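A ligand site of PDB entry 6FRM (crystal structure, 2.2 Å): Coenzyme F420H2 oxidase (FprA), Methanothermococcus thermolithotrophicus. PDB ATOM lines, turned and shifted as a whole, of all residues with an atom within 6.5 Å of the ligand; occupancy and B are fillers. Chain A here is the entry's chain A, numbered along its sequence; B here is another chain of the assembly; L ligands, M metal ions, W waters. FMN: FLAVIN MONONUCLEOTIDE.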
ATOM      1  N   ASP A 265      24.139  17.712 -25.525  1.00  0.00           N
ATOM      2  CA  ASP A 265      23.274  18.232 -24.507  1.00  0.00           C
ATOM      3  C   ASP A 265      23.798  19.620 -24.163  1.00  0.00           C
ATOM      4  O   ASP A 265      24.952  19.908 -24.433  1.00  0.00           O
ATOM      5  CB  ASP A 265      23.021  17.328 -23.299  1.00  0.00           C
ATOM      6  CG  ASP A 265      21.593  17.530 -22.750  1.00  0.00           C
ATOM      7  OD1 ASP A 265      20.961  18.582 -23.080  1.00  0.00           O
ATOM      8  OD2 ASP A 265      21.094  16.616 -22.059  1.00  0.00           O
ATOM      9  N   THR A 266      22.954  20.485 -23.605  1.00  0.00           N
ATOM     10  CA  THR A 266      23.338  21.866 -23.257  1.00  0.00           C
ATOM     11  C   THR A 266      22.460  22.352 -22.112  1.00  0.00           C
ATOM     12  O   THR A 266      21.349  21.864 -21.940  1.00  0.00           O
ATOM     13  CB  THR A 266      23.210  22.776 -24.525  1.00  0.00           C
ATOM     14  OG1 THR A 266      23.904  23.998 -24.341  1.00  0.00           O
ATOM     15  CG2 THR A 266      21.760  23.090 -24.911  1.00  0.00           C
ATOM     16  N   MET A 267      22.947  23.334 -21.359  1.00  0.00           N
ATOM     17  CA  MET A 267      22.239  23.967 -20.253  1.00  0.00           C
ATOM     18  C   MET A 267      21.968  25.401 -20.692  1.00  0.00           C
ATOM     19  O   MET A 267      20.844  25.872 -20.540  1.00  0.00           O
ATOM     20  CB  MET A 267      23.038  23.968 -18.939  1.00  0.00           C
ATOM     21  CG  MET A 267      23.370  22.596 -18.424  1.00  0.00           C
ATOM     22  SD  MET A 267      24.348  22.568 -16.897  1.00  0.00           S
ATOM     23  CE  MET A 267      25.937  23.188 -17.468  1.00  0.00           C
ATOM     24  N   HIS A 268      22.996  26.106 -21.250  1.00  0.00           N
ATOM     25  CA  HIS A 268      22.835  27.501 -21.699  1.00  0.00           C
ATOM     26  C   HIS A 268      22.970  27.750 -23.217  1.00  0.00           C
ATOM     27  O   HIS A 268      23.045  28.904 -23.619  1.00  0.00           O
ATOM     28  CB  HIS A 268      23.776  28.449 -20.953  1.00  0.00           C
ATOM     29  CG  HIS A 268      23.710  28.392 -19.464  1.00  0.00           C
ATOM     30  ND1 HIS A 268      22.543  28.667 -18.753  1.00  0.00           N
ATOM     31  CD2 HIS A 268      24.692  28.139 -18.583  1.00  0.00           C
ATOM     32  CE1 HIS A 268      22.853  28.542 -17.479  1.00  0.00           C
ATOM     33  NE2 HIS A 268      24.134  28.227 -17.328  1.00  0.00           N
ATOM     34  N   GLY A 269      22.974  26.683 -24.026  1.00  0.00           N
ATOM     35  CA  GLY A 269      23.056  26.803 -25.486  1.00  0.00           C
ATOM     36  C   GLY A 269      24.400  26.878 -26.168  1.00  0.00           C
ATOM     37  O   GLY A 269      24.448  26.833 -27.402  1.00  0.00           O
ATOM     38  N   SER A 270      25.521  26.978 -25.410  1.00  0.00           N
ATOM     39  CA  SER A 270      26.855  27.081 -26.048  1.00  0.00           C
ATOM     40  C   SER A 270      27.294  25.793 -26.758  1.00  0.00           C
ATOM     41  O   SER A 270      27.784  25.882 -27.881  1.00  0.00           O
ATOM     42  CB  SER A 270      27.887  27.560 -25.054  1.00  0.00           C
ATOM     43  OG  SER A 270      27.503  28.830 -24.551  1.00  0.00           O
ATOM     44  N   THR A 271      27.094  24.614 -26.124  1.00  0.00           N
ATOM     45  CA  THR A 271      27.427  23.307 -26.718  1.00  0.00           C
ATOM     46  C   THR A 271      26.541  23.084 -27.988  1.00  0.00           C
ATOM     47  O   THR A 271      27.001  22.520 -28.982  1.00  0.00           O
ATOM     48  CB  THR A 271      27.307  22.185 -25.675  1.00  0.00           C
ATOM     49  OG1 THR A 271      28.155  22.508 -24.567  1.00  0.00           O
ATOM     50  CG2 THR A 271      27.720  20.805 -26.233  1.00  0.00           C
ATOM     51  N   GLN A 272      25.279  23.541 -27.927  1.00  0.00           N
ATOM     52  CA  GLN A 272      24.293  23.464 -29.011  1.00  0.00           C
ATOM     53  C   GLN A 272      24.810  24.258 -30.227  1.00  0.00           C
ATOM     54  O   GLN A 272      24.762  23.756 -31.347  1.00  0.00           O
ATOM     55  CB  GLN A 272      22.961  24.039 -28.518  1.00  0.00           C
ATOM     56  CG  GLN A 272      21.864  24.090 -29.566  1.00  0.00           C
ATOM     57  CD  GLN A 272      20.562  24.416 -28.921  1.00  0.00           C
ATOM     58  OE1 GLN A 272      20.386  25.509 -28.388  1.00  0.00           O
ATOM     59  NE2 GLN A 272      19.648  23.485 -28.913  1.00  0.00           N
ATOM     60  N   ALA A 316      28.844  17.941 -24.671  1.00  0.00           N
ATOM     61  CA  ALA A 316      28.104  18.237 -23.437  1.00  0.00           C
ATOM     62  C   ALA A 316      28.867  19.245 -22.611  1.00  0.00           C
ATOM     63  O   ALA A 316      30.098  19.214 -22.618  1.00  0.00           O
ATOM     64  CB  ALA A 316      27.901  16.944 -22.616  1.00  0.00           C
ATOM     65  N   PRO A 317      28.177  20.122 -21.858  1.00  0.00           N
ATOM     66  CA  PRO A 317      28.919  21.066 -21.007  1.00  0.00           C
ATOM     67  C   PRO A 317      29.487  20.365 -19.750  1.00  0.00           C
ATOM     68  O   PRO A 317      29.129  19.222 -19.468  1.00  0.00           O
ATOM     69  CB  PRO A 317      27.839  22.078 -20.608  1.00  0.00           C
ATOM     70  CG  PRO A 317      26.564  21.319 -20.630  1.00  0.00           C
ATOM     71  CD  PRO A 317      26.715  20.306 -21.717  1.00  0.00           C
ATOM     72  N   THR A 318      30.363  21.046 -19.006  1.00  0.00           N
ATOM     73  CA  THR A 318      30.946  20.508 -17.774  1.00  0.00           C
ATOM     74  C   THR A 318      30.083  20.987 -16.611  1.00  0.00           C
ATOM     75  O   THR A 318      29.714  22.166 -16.543  1.00  0.00           O
ATOM     76  CB  THR A 318      32.416  20.963 -17.578  1.00  0.00           C
ATOM     77  OG1 THR A 318      33.198  20.490 -18.680  1.00  0.00           O
ATOM     78  CG2 THR A 318      33.027  20.427 -16.273  1.00  0.00           C
ATOM     79  N   ILE A 319      29.759  20.069 -15.703  1.00  0.00           N
ATOM     80  CA  ILE A 319      28.964  20.327 -14.506  1.00  0.00           C
ATOM     81  C   ILE A 319      29.648  19.557 -13.378  1.00  0.00           C
ATOM     82  O   ILE A 319      29.708  18.333 -13.415  1.00  0.00           O
ATOM     83  CB  ILE A 319      27.444  20.005 -14.703  1.00  0.00           C
ATOM     84  CG1 ILE A 319      26.661  20.154 -13.382  1.00  0.00           C
ATOM     85  CG2 ILE A 319      27.210  18.640 -15.360  1.00  0.00           C
ATOM     86  CD1 ILE A 319      25.113  20.260 -13.579  1.00  0.00           C
ATOM     87  N   TYR A 320      30.208  20.286 -12.405  1.00  0.00           N
ATOM     88  CA  TYR A 320      30.927  19.737 -11.259  1.00  0.00           C
ATOM     89  C   TYR A 320      31.997  18.710 -11.701  1.00  0.00           C
ATOM     90  O   TYR A 320      32.019  17.561 -11.227  1.00  0.00           O
ATOM     91  CB  TYR A 320      29.969  19.215 -10.183  1.00  0.00           C
ATOM     92  CG  TYR A 320      29.084  20.312  -9.644  1.00  0.00           C
ATOM     93  CD1 TYR A 320      29.634  21.487  -9.118  1.00  0.00           C
ATOM     94  CD2 TYR A 320      27.692  20.191  -9.670  1.00  0.00           C
ATOM     95  CE1 TYR A 320      28.830  22.502  -8.616  1.00  0.00           C
ATOM     96  CE2 TYR A 320      26.875  21.208  -9.173  1.00  0.00           C
ATOM     97  CZ  TYR A 320      27.450  22.362  -8.644  1.00  0.00           C
ATOM     98  OH  TYR A 320      26.673  23.374  -8.155  1.00  0.00           O
ATOM     99  N   ASP A 321      32.880  19.162 -12.646  1.00  0.00           N
ATOM    100  CA  ASP A 321      34.017  18.424 -13.256  1.00  0.00           C
ATOM    101  C   ASP A 321      33.621  17.252 -14.172  1.00  0.00           C
ATOM    102  O   ASP A 321      34.489  16.566 -14.703  1.00  0.00           O
ATOM    103  CB  ASP A 321      34.996  17.921 -12.156  1.00  0.00           C
ATOM    104  CG  ASP A 321      35.425  18.973 -11.137  1.00  0.00           C
ATOM    105  OD1 ASP A 321      35.698  20.119 -11.544  1.00  0.00           O
ATOM    106  OD2 ASP A 321      35.502  18.646  -9.935  1.00  0.00           O
ATOM    107  N   GLU A 322      32.321  17.032 -14.358  1.00  0.00           N
ATOM    108  CA  GLU A 322      31.854  15.918 -15.173  1.00  0.00           C
ATOM    109  C   GLU A 322      31.038  16.385 -16.365  1.00  0.00           C
ATOM    110  O   GLU A 322      30.498  17.479 -16.311  1.00  0.00           O
ATOM    111  CB  GLU A 322      30.951  14.991 -14.292  1.00  0.00           C
ATOM    112  CG  GLU A 322      31.627  14.387 -13.076  1.00  0.00           C
ATOM    113  CD  GLU A 322      32.735  13.388 -13.352  1.00  0.00           C
ATOM    114  OE1 GLU A 322      33.628  13.254 -12.480  1.00  0.00           O
ATOM    115  OE2 GLU A 322      32.695  12.719 -14.407  1.00  0.00           O
ATOM    116  N   GLY A 352      32.488  20.432 -26.088  1.00  0.00           N
ATOM    117  CA  GLY A 352      31.704  21.024 -25.024  1.00  0.00           C
ATOM    118  C   GLY A 352      32.178  22.381 -24.577  1.00  0.00           C
ATOM    119  O   GLY A 352      33.294  22.810 -24.902  1.00  0.00           O
ATOM    120  N   SER A 353      31.312  23.074 -23.852  1.00  0.00           N
ATOM    121  CA  SER A 353      31.617  24.381 -23.297  1.00  0.00           C
ATOM    122  C   SER A 353      31.829  24.188 -21.781  1.00  0.00           C
ATOM    123  O   SER A 353      31.343  23.216 -21.198  1.00  0.00           O
ATOM    124  CB  SER A 353      30.472  25.350 -23.578  1.00  0.00           C
ATOM    125  OG  SER A 353      30.748  26.609 -23.007  1.00  0.00           O
ATOM    126  N   MET A 354      32.577  25.100 -21.158  1.00  0.00           N
ATOM    127  CA  MET A 354      32.862  25.048 -19.730  1.00  0.00           C
ATOM    128  C   MET A 354      32.995  26.473 -19.187  1.00  0.00           C
ATOM    129  O   MET A 354      33.126  27.430 -19.958  1.00  0.00           O
ATOM    130  CB  MET A 354      34.068  24.142 -19.395  1.00  0.00           C
ATOM    131  CG  MET A 354      35.330  24.466 -20.167  1.00  0.00           C
ATOM    132  SD  MET A 354      36.330  25.765 -19.427  1.00  0.00           S
ATOM    133  CE  MET A 354      37.582  25.928 -20.641  1.00  0.00           C
ATOM    134  N   GLY A 355      32.959  26.616 -17.871  1.00  0.00           N
ATOM    135  CA  GLY A 355      33.057  27.920 -17.246  1.00  0.00           C
ATOM    136  C   GLY A 355      34.122  28.099 -16.181  1.00  0.00           C
ATOM    137  O   GLY A 355      34.282  29.195 -15.670  1.00  0.00           O
ATOM    138  N   GLY A 356      34.844  27.020 -15.860  1.00  0.00           N
ATOM    139  CA  GLY A 356      35.903  27.035 -14.866  1.00  0.00           C
ATOM    140  C   GLY A 356      37.098  26.219 -15.292  1.00  0.00           C
ATOM    141  O   GLY A 356      37.831  26.586 -16.223  1.00  0.00           O
ATOM    142  N   ASN A 357      37.294  25.087 -14.609  1.00  0.00           N
ATOM    143  CA  ASN A 357      38.404  24.177 -14.890  1.00  0.00           C
ATOM    144  C   ASN A 357      38.157  23.196 -16.040  1.00  0.00           C
ATOM    145  O   ASN A 357      39.102  22.631 -16.575  1.00  0.00           O
ATOM    146  CB  ASN A 357      38.812  23.408 -13.626  1.00  0.00           C
ATOM    147  CG  ASN A 357      39.431  24.270 -12.558  1.00  0.00           C
ATOM    148  OD1 ASN A 357      40.271  25.151 -12.834  1.00  0.00           O
ATOM    149  ND2 ASN A 357      39.039  24.033 -11.316  1.00  0.00           N
ATOM    150  N   GLY A 358      36.881  22.999 -16.389  1.00  0.00           N
ATOM    151  CA  GLY A 358      36.491  22.078 -17.448  1.00  0.00           C
ATOM    152  C   GLY A 358      36.697  20.621 -17.053  1.00  0.00           C
ATOM    153  O   GLY A 358      36.653  20.279 -15.860  1.00  0.00           O
ATOM    154  N   GLY A 359      36.923  19.774 -18.050  1.00  0.00           N
ATOM    155  CA  GLY A 359      37.139  18.350 -17.859  1.00  0.00           C
ATOM    156  C   GLY A 359      36.101  17.423 -18.465  1.00  0.00           C
ATOM    157  O   GLY A 359      36.375  16.237 -18.635  1.00  0.00           O
ATOM    158  N   LEU A 381      35.686  24.749 -25.069  1.00  0.00           N
ATOM    159  CA  LEU A 381      35.838  26.200 -25.041  1.00  0.00           C
ATOM    160  C   LEU A 381      35.186  26.800 -23.788  1.00  0.00           C
ATOM    161  O   LEU A 381      34.463  26.117 -23.071  1.00  0.00           O
ATOM    162  CB  LEU A 381      35.382  26.903 -26.352  1.00  0.00           C
ATOM    163  CG  LEU A 381      34.009  26.574 -26.928  1.00  0.00           C
ATOM    164  CD1 LEU A 381      32.879  27.260 -26.149  1.00  0.00           C
ATOM    165  CD2 LEU A 381      33.952  26.997 -28.372  1.00  0.00           C
ATOM    166  N   TYR A 382      35.455  28.080 -23.552  1.00  0.00           N
ATOM    167  CA  TYR A 382      34.988  28.854 -22.407  1.00  0.00           C
ATOM    168  C   TYR A 382      33.702  29.604 -22.727  1.00  0.00           C
ATOM    169  O   TYR A 382      33.671  30.406 -23.639  1.00  0.00           O
ATOM    170  CB  TYR A 382      36.117  29.820 -22.014  1.00  0.00           C
ATOM    171  CG  TYR A 382      35.966  30.642 -20.748  1.00  0.00           C
ATOM    172  CD1 TYR A 382      35.675  30.034 -19.534  1.00  0.00           C
ATOM    173  CD2 TYR A 382      36.174  32.015 -20.765  1.00  0.00           C
ATOM    174  CE1 TYR A 382      35.576  30.790 -18.362  1.00  0.00           C
ATOM    175  CE2 TYR A 382      36.070  32.779 -19.597  1.00  0.00           C
ATOM    176  CZ  TYR A 382      35.771  32.167 -18.407  1.00  0.00           C
ATOM    177  OH  TYR A 382      35.668  32.934 -17.261  1.00  0.00           O
ATOM    178  N   TYR A 383      32.649  29.328 -21.963  1.00  0.00           N
ATOM    179  CA  TYR A 383      31.331  29.933 -22.073  1.00  0.00           C
ATOM    180  C   TYR A 383      30.792  30.011 -23.520  1.00  0.00           C
ATOM    181  O   TYR A 383      30.803  29.011 -24.228  1.00  0.00           O
ATOM    182  CB  TYR A 383      31.302  31.293 -21.384  1.00  0.00           C
ATOM    183  CG  TYR A 383      31.393  31.214 -19.874  1.00  0.00           C
ATOM    184  CD1 TYR A 383      30.527  30.399 -19.148  1.00  0.00           C
ATOM    185  CD2 TYR A 383      32.312  31.980 -19.166  1.00  0.00           C
ATOM    186  CE1 TYR A 383      30.595  30.335 -17.758  1.00  0.00           C
ATOM    187  CE2 TYR A 383      32.378  31.938 -17.783  1.00  0.00           C
ATOM    188  CZ  TYR A 383      31.515  31.104 -17.072  1.00  0.00           C
ATOM    189  OH  TYR A 383      31.600  31.053 -15.703  1.00  0.00           O
ATOM    190  N   VAL A 384      30.311  31.176 -23.938  1.00  0.00           N
ATOM    191  CA  VAL A 384      29.743  31.410 -25.267  1.00  0.00           C
ATOM    192  C   VAL A 384      30.824  31.397 -26.369  1.00  0.00           C
ATOM    193  O   VAL A 384      31.818  32.113 -26.243  1.00  0.00           O
ATOM    194  CB  VAL A 384      28.869  32.698 -25.285  1.00  0.00           C
ATOM    195  CG1 VAL A 384      28.167  32.881 -26.627  1.00  0.00           C
ATOM    196  CG2 VAL A 384      27.836  32.671 -24.167  1.00  0.00           C
ATOM    197  N   TYR B  25      15.520  23.355 -15.445  1.00  0.00           N
ATOM    198  CA  TYR B  25      16.676  24.248 -15.468  1.00  0.00           C
ATOM    199  C   TYR B  25      17.902  23.391 -15.165  1.00  0.00           C
ATOM    200  O   TYR B  25      17.993  22.855 -14.068  1.00  0.00           O
ATOM    201  CB  TYR B  25      16.507  25.435 -14.495  1.00  0.00           C
ATOM    202  CG  TYR B  25      17.617  26.465 -14.595  1.00  0.00           C
ATOM    203  CD1 TYR B  25      18.099  26.874 -15.831  1.00  0.00           C
ATOM    204  CD2 TYR B  25      18.176  27.023 -13.450  1.00  0.00           C
ATOM    205  CE1 TYR B  25      19.132  27.820 -15.929  1.00  0.00           C
ATOM    206  CE2 TYR B  25      19.210  27.964 -13.535  1.00  0.00           C
ATOM    207  CZ  TYR B  25      19.679  28.360 -14.781  1.00  0.00           C
ATOM    208  OH  TYR B  25      20.687  29.290 -14.881  1.00  0.00           O
ATOM    209  N   HIS B  26      18.808  23.243 -16.146  1.00  0.00           N
ATOM    210  CA  HIS B  26      20.032  22.425 -16.095  1.00  0.00           C
ATOM    211  C   HIS B  26      19.771  21.030 -15.487  1.00  0.00           C
ATOM    212  O   HIS B  26      20.480  20.568 -14.590  1.00  0.00           O
ATOM    213  CB  HIS B  26      21.255  23.138 -15.454  1.00  0.00           C
ATOM    214  CG  HIS B  26      21.045  23.727 -14.099  1.00  0.00           C
ATOM    215  ND1 HIS B  26      20.812  22.934 -12.997  1.00  0.00           N
ATOM    216  CD2 HIS B  26      21.085  25.022 -13.707  1.00  0.00           C
ATOM    217  CE1 HIS B  26      20.689  23.767 -11.975  1.00  0.00           C
ATOM    218  NE2 HIS B  26      20.842  25.035 -12.346  1.00  0.00           N
ATOM    219  N   GLU B  86      26.729  33.804 -14.029  1.00  0.00           N
ATOM    220  CA  GLU B  86      25.596  33.003 -14.518  1.00  0.00           C
ATOM    221  C   GLU B  86      24.507  33.867 -15.186  1.00  0.00           C
ATOM    222  O   GLU B  86      24.013  34.792 -14.553  1.00  0.00           O
ATOM    223  CB  GLU B  86      24.973  32.198 -13.374  1.00  0.00           C
ATOM    224  CG  GLU B  86      25.485  30.784 -13.218  1.00  0.00           C
ATOM    225  CD  GLU B  86      24.630  29.731 -13.894  1.00  0.00           C
ATOM    226  OE1 GLU B  86      24.848  29.496 -15.106  1.00  0.00           O
ATOM    227  OE2 GLU B  86      23.791  29.102 -13.207  1.00  0.00           O
ATOM    228  N   LYS B  87      24.159  33.554 -16.454  1.00  0.00           N
ATOM    229  CA  LYS B  87      23.164  34.326 -17.217  1.00  0.00           C
ATOM    230  C   LYS B  87      21.794  34.478 -16.560  1.00  0.00           C
ATOM    231  O   LYS B  87      21.080  35.403 -16.918  1.00  0.00           O
ATOM    232  CB  LYS B  87      23.019  33.855 -18.670  1.00  0.00           C
ATOM    233  CG  LYS B  87      22.391  32.506 -18.937  1.00  0.00           C
ATOM    234  CD  LYS B  87      22.613  32.268 -20.419  1.00  0.00           C
ATOM    235  CE  LYS B  87      21.470  31.649 -21.173  1.00  0.00           C
ATOM    236  NZ  LYS B  87      21.814  31.509 -22.606  1.00  0.00           N
ATOM    237  N   HIS B 118      30.345  36.165 -22.215  1.00  0.00           N
ATOM    238  CA  HIS B 118      28.902  35.976 -22.366  1.00  0.00           C
ATOM    239  C   HIS B 118      28.294  37.101 -23.201  1.00  0.00           C
ATOM    240  O   HIS B 118      27.453  36.821 -24.049  1.00  0.00           O
ATOM    241  CB  HIS B 118      28.197  36.017 -20.999  1.00  0.00           C
ATOM    242  CG  HIS B 118      28.178  34.729 -20.266  1.00  0.00           C
ATOM    243  ND1 HIS B 118      27.310  33.721 -20.601  1.00  0.00           N
ATOM    244  CD2 HIS B 118      28.920  34.341 -19.207  1.00  0.00           C
ATOM    245  CE1 HIS B 118      27.551  32.735 -19.755  1.00  0.00           C
ATOM    246  NE2 HIS B 118      28.506  33.056 -18.886  1.00  0.00           N
ATOM    247  N   ASN B 202      21.221  19.208  -5.175  1.00  0.00           N
ATOM    248  CA  ASN B 202      21.598  19.361  -6.569  1.00  0.00           C
ATOM    249  C   ASN B 202      22.684  20.363  -6.853  1.00  0.00           C
ATOM    250  O   ASN B 202      23.336  20.246  -7.897  1.00  0.00           O
ATOM    251  CB  ASN B 202      20.367  19.727  -7.352  1.00  0.00           C
ATOM    252  CG  ASN B 202      19.400  18.586  -7.501  1.00  0.00           C
ATOM    253  OD1 ASN B 202      19.507  17.822  -8.440  1.00  0.00           O
ATOM    254  ND2 ASN B 202      18.465  18.417  -6.561  1.00  0.00           N
ATOM    255  N   LEU B 203      22.884  21.345  -5.978  1.00  0.00           N
ATOM    256  CA  LEU B 203      23.886  22.380  -6.244  1.00  0.00           C
ATOM    257  C   LEU B 203      24.974  22.621  -5.212  1.00  0.00           C
ATOM    258  O   LEU B 203      26.025  23.138  -5.585  1.00  0.00           O
ATOM    259  CB  LEU B 203      23.131  23.722  -6.504  1.00  0.00           C
ATOM    260  CG  LEU B 203      22.179  23.720  -7.710  1.00  0.00           C
ATOM    261  CD1 LEU B 203      21.132  24.776  -7.598  1.00  0.00           C
ATOM    262  CD2 LEU B 203      22.924  23.830  -9.026  1.00  0.00           C
HETATM  263  N1  FMN L   1      32.317  24.837 -15.352  1.00  0.00           N
HETATM  264  C2  FMN L   1      33.473  24.197 -15.061  1.00  0.00           C
HETATM  265  O2  FMN L   1      34.506  24.502 -15.688  1.00  0.00           O
HETATM  266  N3  FMN L   1      33.561  23.247 -14.108  1.00  0.00           N
HETATM  267  C4  FMN L   1      32.495  22.868 -13.381  1.00  0.00           C
HETATM  268  O4  FMN L   1      32.607  21.983 -12.506  1.00  0.00           O
HETATM  269  C4A FMN L   1      31.199  23.515 -13.639  1.00  0.00           C
HETATM  270  N5  FMN L   1      30.080  23.186 -12.954  1.00  0.00           N
HETATM  271  C5A FMN L   1      28.903  23.799 -13.221  1.00  0.00           C
HETATM  272  C6  FMN L   1      27.766  23.439 -12.499  1.00  0.00           C
HETATM  273  C7  FMN L   1      26.543  24.065 -12.762  1.00  0.00           C
HETATM  274  C7M FMN L   1      25.320  23.681 -11.981  1.00  0.00           C
HETATM  275  C8  FMN L   1      26.464  25.109 -13.818  1.00  0.00           C
HETATM  276  C8M FMN L   1      25.140  25.782 -14.093  1.00  0.00           C
HETATM  277  C9  FMN L   1      27.590  25.467 -14.532  1.00  0.00           C
HETATM  278  C9A FMN L   1      28.807  24.849 -14.273  1.00  0.00           C
HETATM  279  N10 FMN L   1      29.960  25.204 -15.000  1.00  0.00           N
HETATM  280  C10 FMN L   1      31.164  24.546 -14.700  1.00  0.00           C
HETATM  281  C1' FMN L   1      29.903  26.230 -16.043  1.00  0.00           C
HETATM  282  C2' FMN L   1      29.371  25.615 -17.337  1.00  0.00           C
HETATM  283  O2' FMN L   1      30.258  24.573 -17.763  1.00  0.00           O
HETATM  284  C3' FMN L   1      29.253  26.668 -18.429  1.00  0.00           C
HETATM  285  O3' FMN L   1      28.103  27.481 -18.195  1.00  0.00           O
HETATM  286  C4' FMN L   1      29.146  26.018 -19.804  1.00  0.00           C
HETATM  287  O4' FMN L   1      29.554  26.950 -20.811  1.00  0.00           O
HETATM  288  C5' FMN L   1      27.719  25.565 -20.074  1.00  0.00           C
HETATM  289  O5' FMN L   1      27.622  25.078 -21.410  1.00  0.00           O
HETATM  290  P   FMN L   1      26.210  25.116 -22.199  1.00  0.00           P
HETATM  291  O1P FMN L   1      26.015  26.580 -22.517  1.00  0.00           O
HETATM  292  O2P FMN L   1      26.452  24.237 -23.410  1.00  0.00           O
HETATM  293  O3P FMN L   1      25.227  24.552 -21.204  1.00  0.00           O
HETATM  294 FE    FE M   1      23.742  30.733 -11.117  1.00  0.00          FE
HETATM  295  O   HOH W   1      34.069  22.738  -9.957  1.00  0.00           O
HETATM  296  O   HOH W   2      27.281  28.914 -21.856  1.00  0.00           O
HETATM  297  O   HOH W   3      35.808  21.744 -13.693  1.00  0.00           O
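CB of Pro 317 touches O5' of the ligand (3.1 Å).
CA of Ile 319 touches N5 of the ligand, at 3.4 Å.
Met 354 touches the ligand (CA to O2', 3.3 Å).
Tyr 383 touches the ligand (CA to O4', 3.7 Å).
Glu 86 of chain B touches the ligand (OE2 to C8M, 3.7 Å).
Leu 203 of chain B touches the ligand (CD2 to C7M, 3.8 Å).
Hydrophobic or aromatic side chains that line the ligand: Met 267, His 268, Pro 317, Ile 319, Met 354, Tyr 383 and Leu 203 of chain B.
Of the 34 residues printed, 20 come within 4 Å of the ligand.
The nearest printed residue that does not touch the ligand is His 26 of chain B (4.1 Å).
Water W3 lies within hydrogen-bond range of the side-chain carboxylate of Asp 321 (2.7 Å), a nitrogen (N3) of the ligand (2.7 Å) and the backbone carbonyl oxygen of Gly 358 (2.7 Å).
Water W2 bridges the side-chain hydroxyl (OG) of Ser 270 and an oxygen (O1P) of the ligand.
Water W1 bridges an oxygen (O4) of the ligand (3.0 Å) and the side-chain carboxylate (OD1) of Asp 321 (3.5 Å).
OG1 of Thr 271 sits at hydrogen-bond distance from O2P of the ligand (2.7 Å).
The backbone NH (N) of Asn 357 sits at hydrogen-bond distance from an oxygen (O2) of the ligand (3.0 Å).
The backbone NH of Gly 269 lies within hydrogen-bond range of an oxygen (O1P) of the ligand (3.4 Å).
An oxygen (O2P) of the ligand lies within hydrogen-bond range of the side-chain hydroxyl (OG1) of Thr 266 (2.7 Å).
The backbone NH (N) of Gly 356 lies within hydrogen-bond range of an oxygen (O2) of the ligand, at 2.5 Å.
The backbone NH of Asp 321 sits at hydrogen-bond distance from an oxygen (O4) of the ligand (2.8 Å).
The backbone NH (N) of Ser 270 is in hydrogen-bond range of an oxygen (O1P) of the ligand (3.0 Å).
The backbone NH (N) of Thr 271 sits at hydrogen-bond distance from an oxygen (O2P) of the ligand, 2.8 Å away.
An oxygen (O4') of the ligand lies within hydrogen-bond range of the side-chain hydroxyl (OG) of Ser 353.
An oxygen (O2') of the ligand lies within hydrogen-bond range of the backbone carbonyl oxygen (O) of Thr 318 (2.8 Å).
N of Gly 355 is in hydrogen-bond range of N1 of the ligand (3.1 Å).
O1P of the ligand lies close to OG of Ser 270.
N of Gly 358 is in hydrogen-bond range of O2 of the ligand (2.9 Å).
An oxygen (O4) of the ligand is in hydrogen-bond range of the backbone NH (N) of Tyr 320 (2.9 Å).
The backbone NH (N) of His 268 is in hydrogen-bond range of an oxygen (O3P) of the ligand (2.7 Å).
The backbone NH of Met 267 sits at hydrogen-bond distance from an oxygen (O3P) of the ligand.
O of Tyr 383 lies within hydrogen-bond range of OG of Ser 353 (2.7 Å).
The backbone carbonyl oxygen (O) of Gly 355 is in hydrogen-bond range of the side-chain hydroxyl (OH) of Tyr 383 (3.3 Å).
OG1 of Thr 266 lies within hydrogen-bond range of N of Gly 269, 2.9 Å away.
OH of Tyr 320 is in hydrogen-bond range of O of Leu 203 of chain B, 2.7 Å away.
NZ of Lys 87 of chain B sits at hydrogen-bond distance from O of His 268, 3.1 Å away.
NE2 of His 268 sits at hydrogen-bond distance from OE1 of Glu 86 of chain B (2.7 Å).
The side-chain hydroxyl (OG) of Ser 270 is in hydrogen-bond range of the backbone carbonyl oxygen (O) of Tyr 383 (3.3 Å).
N of Ser 353 sits at hydrogen-bond distance from OG1 of Thr 271 (3.3 Å).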
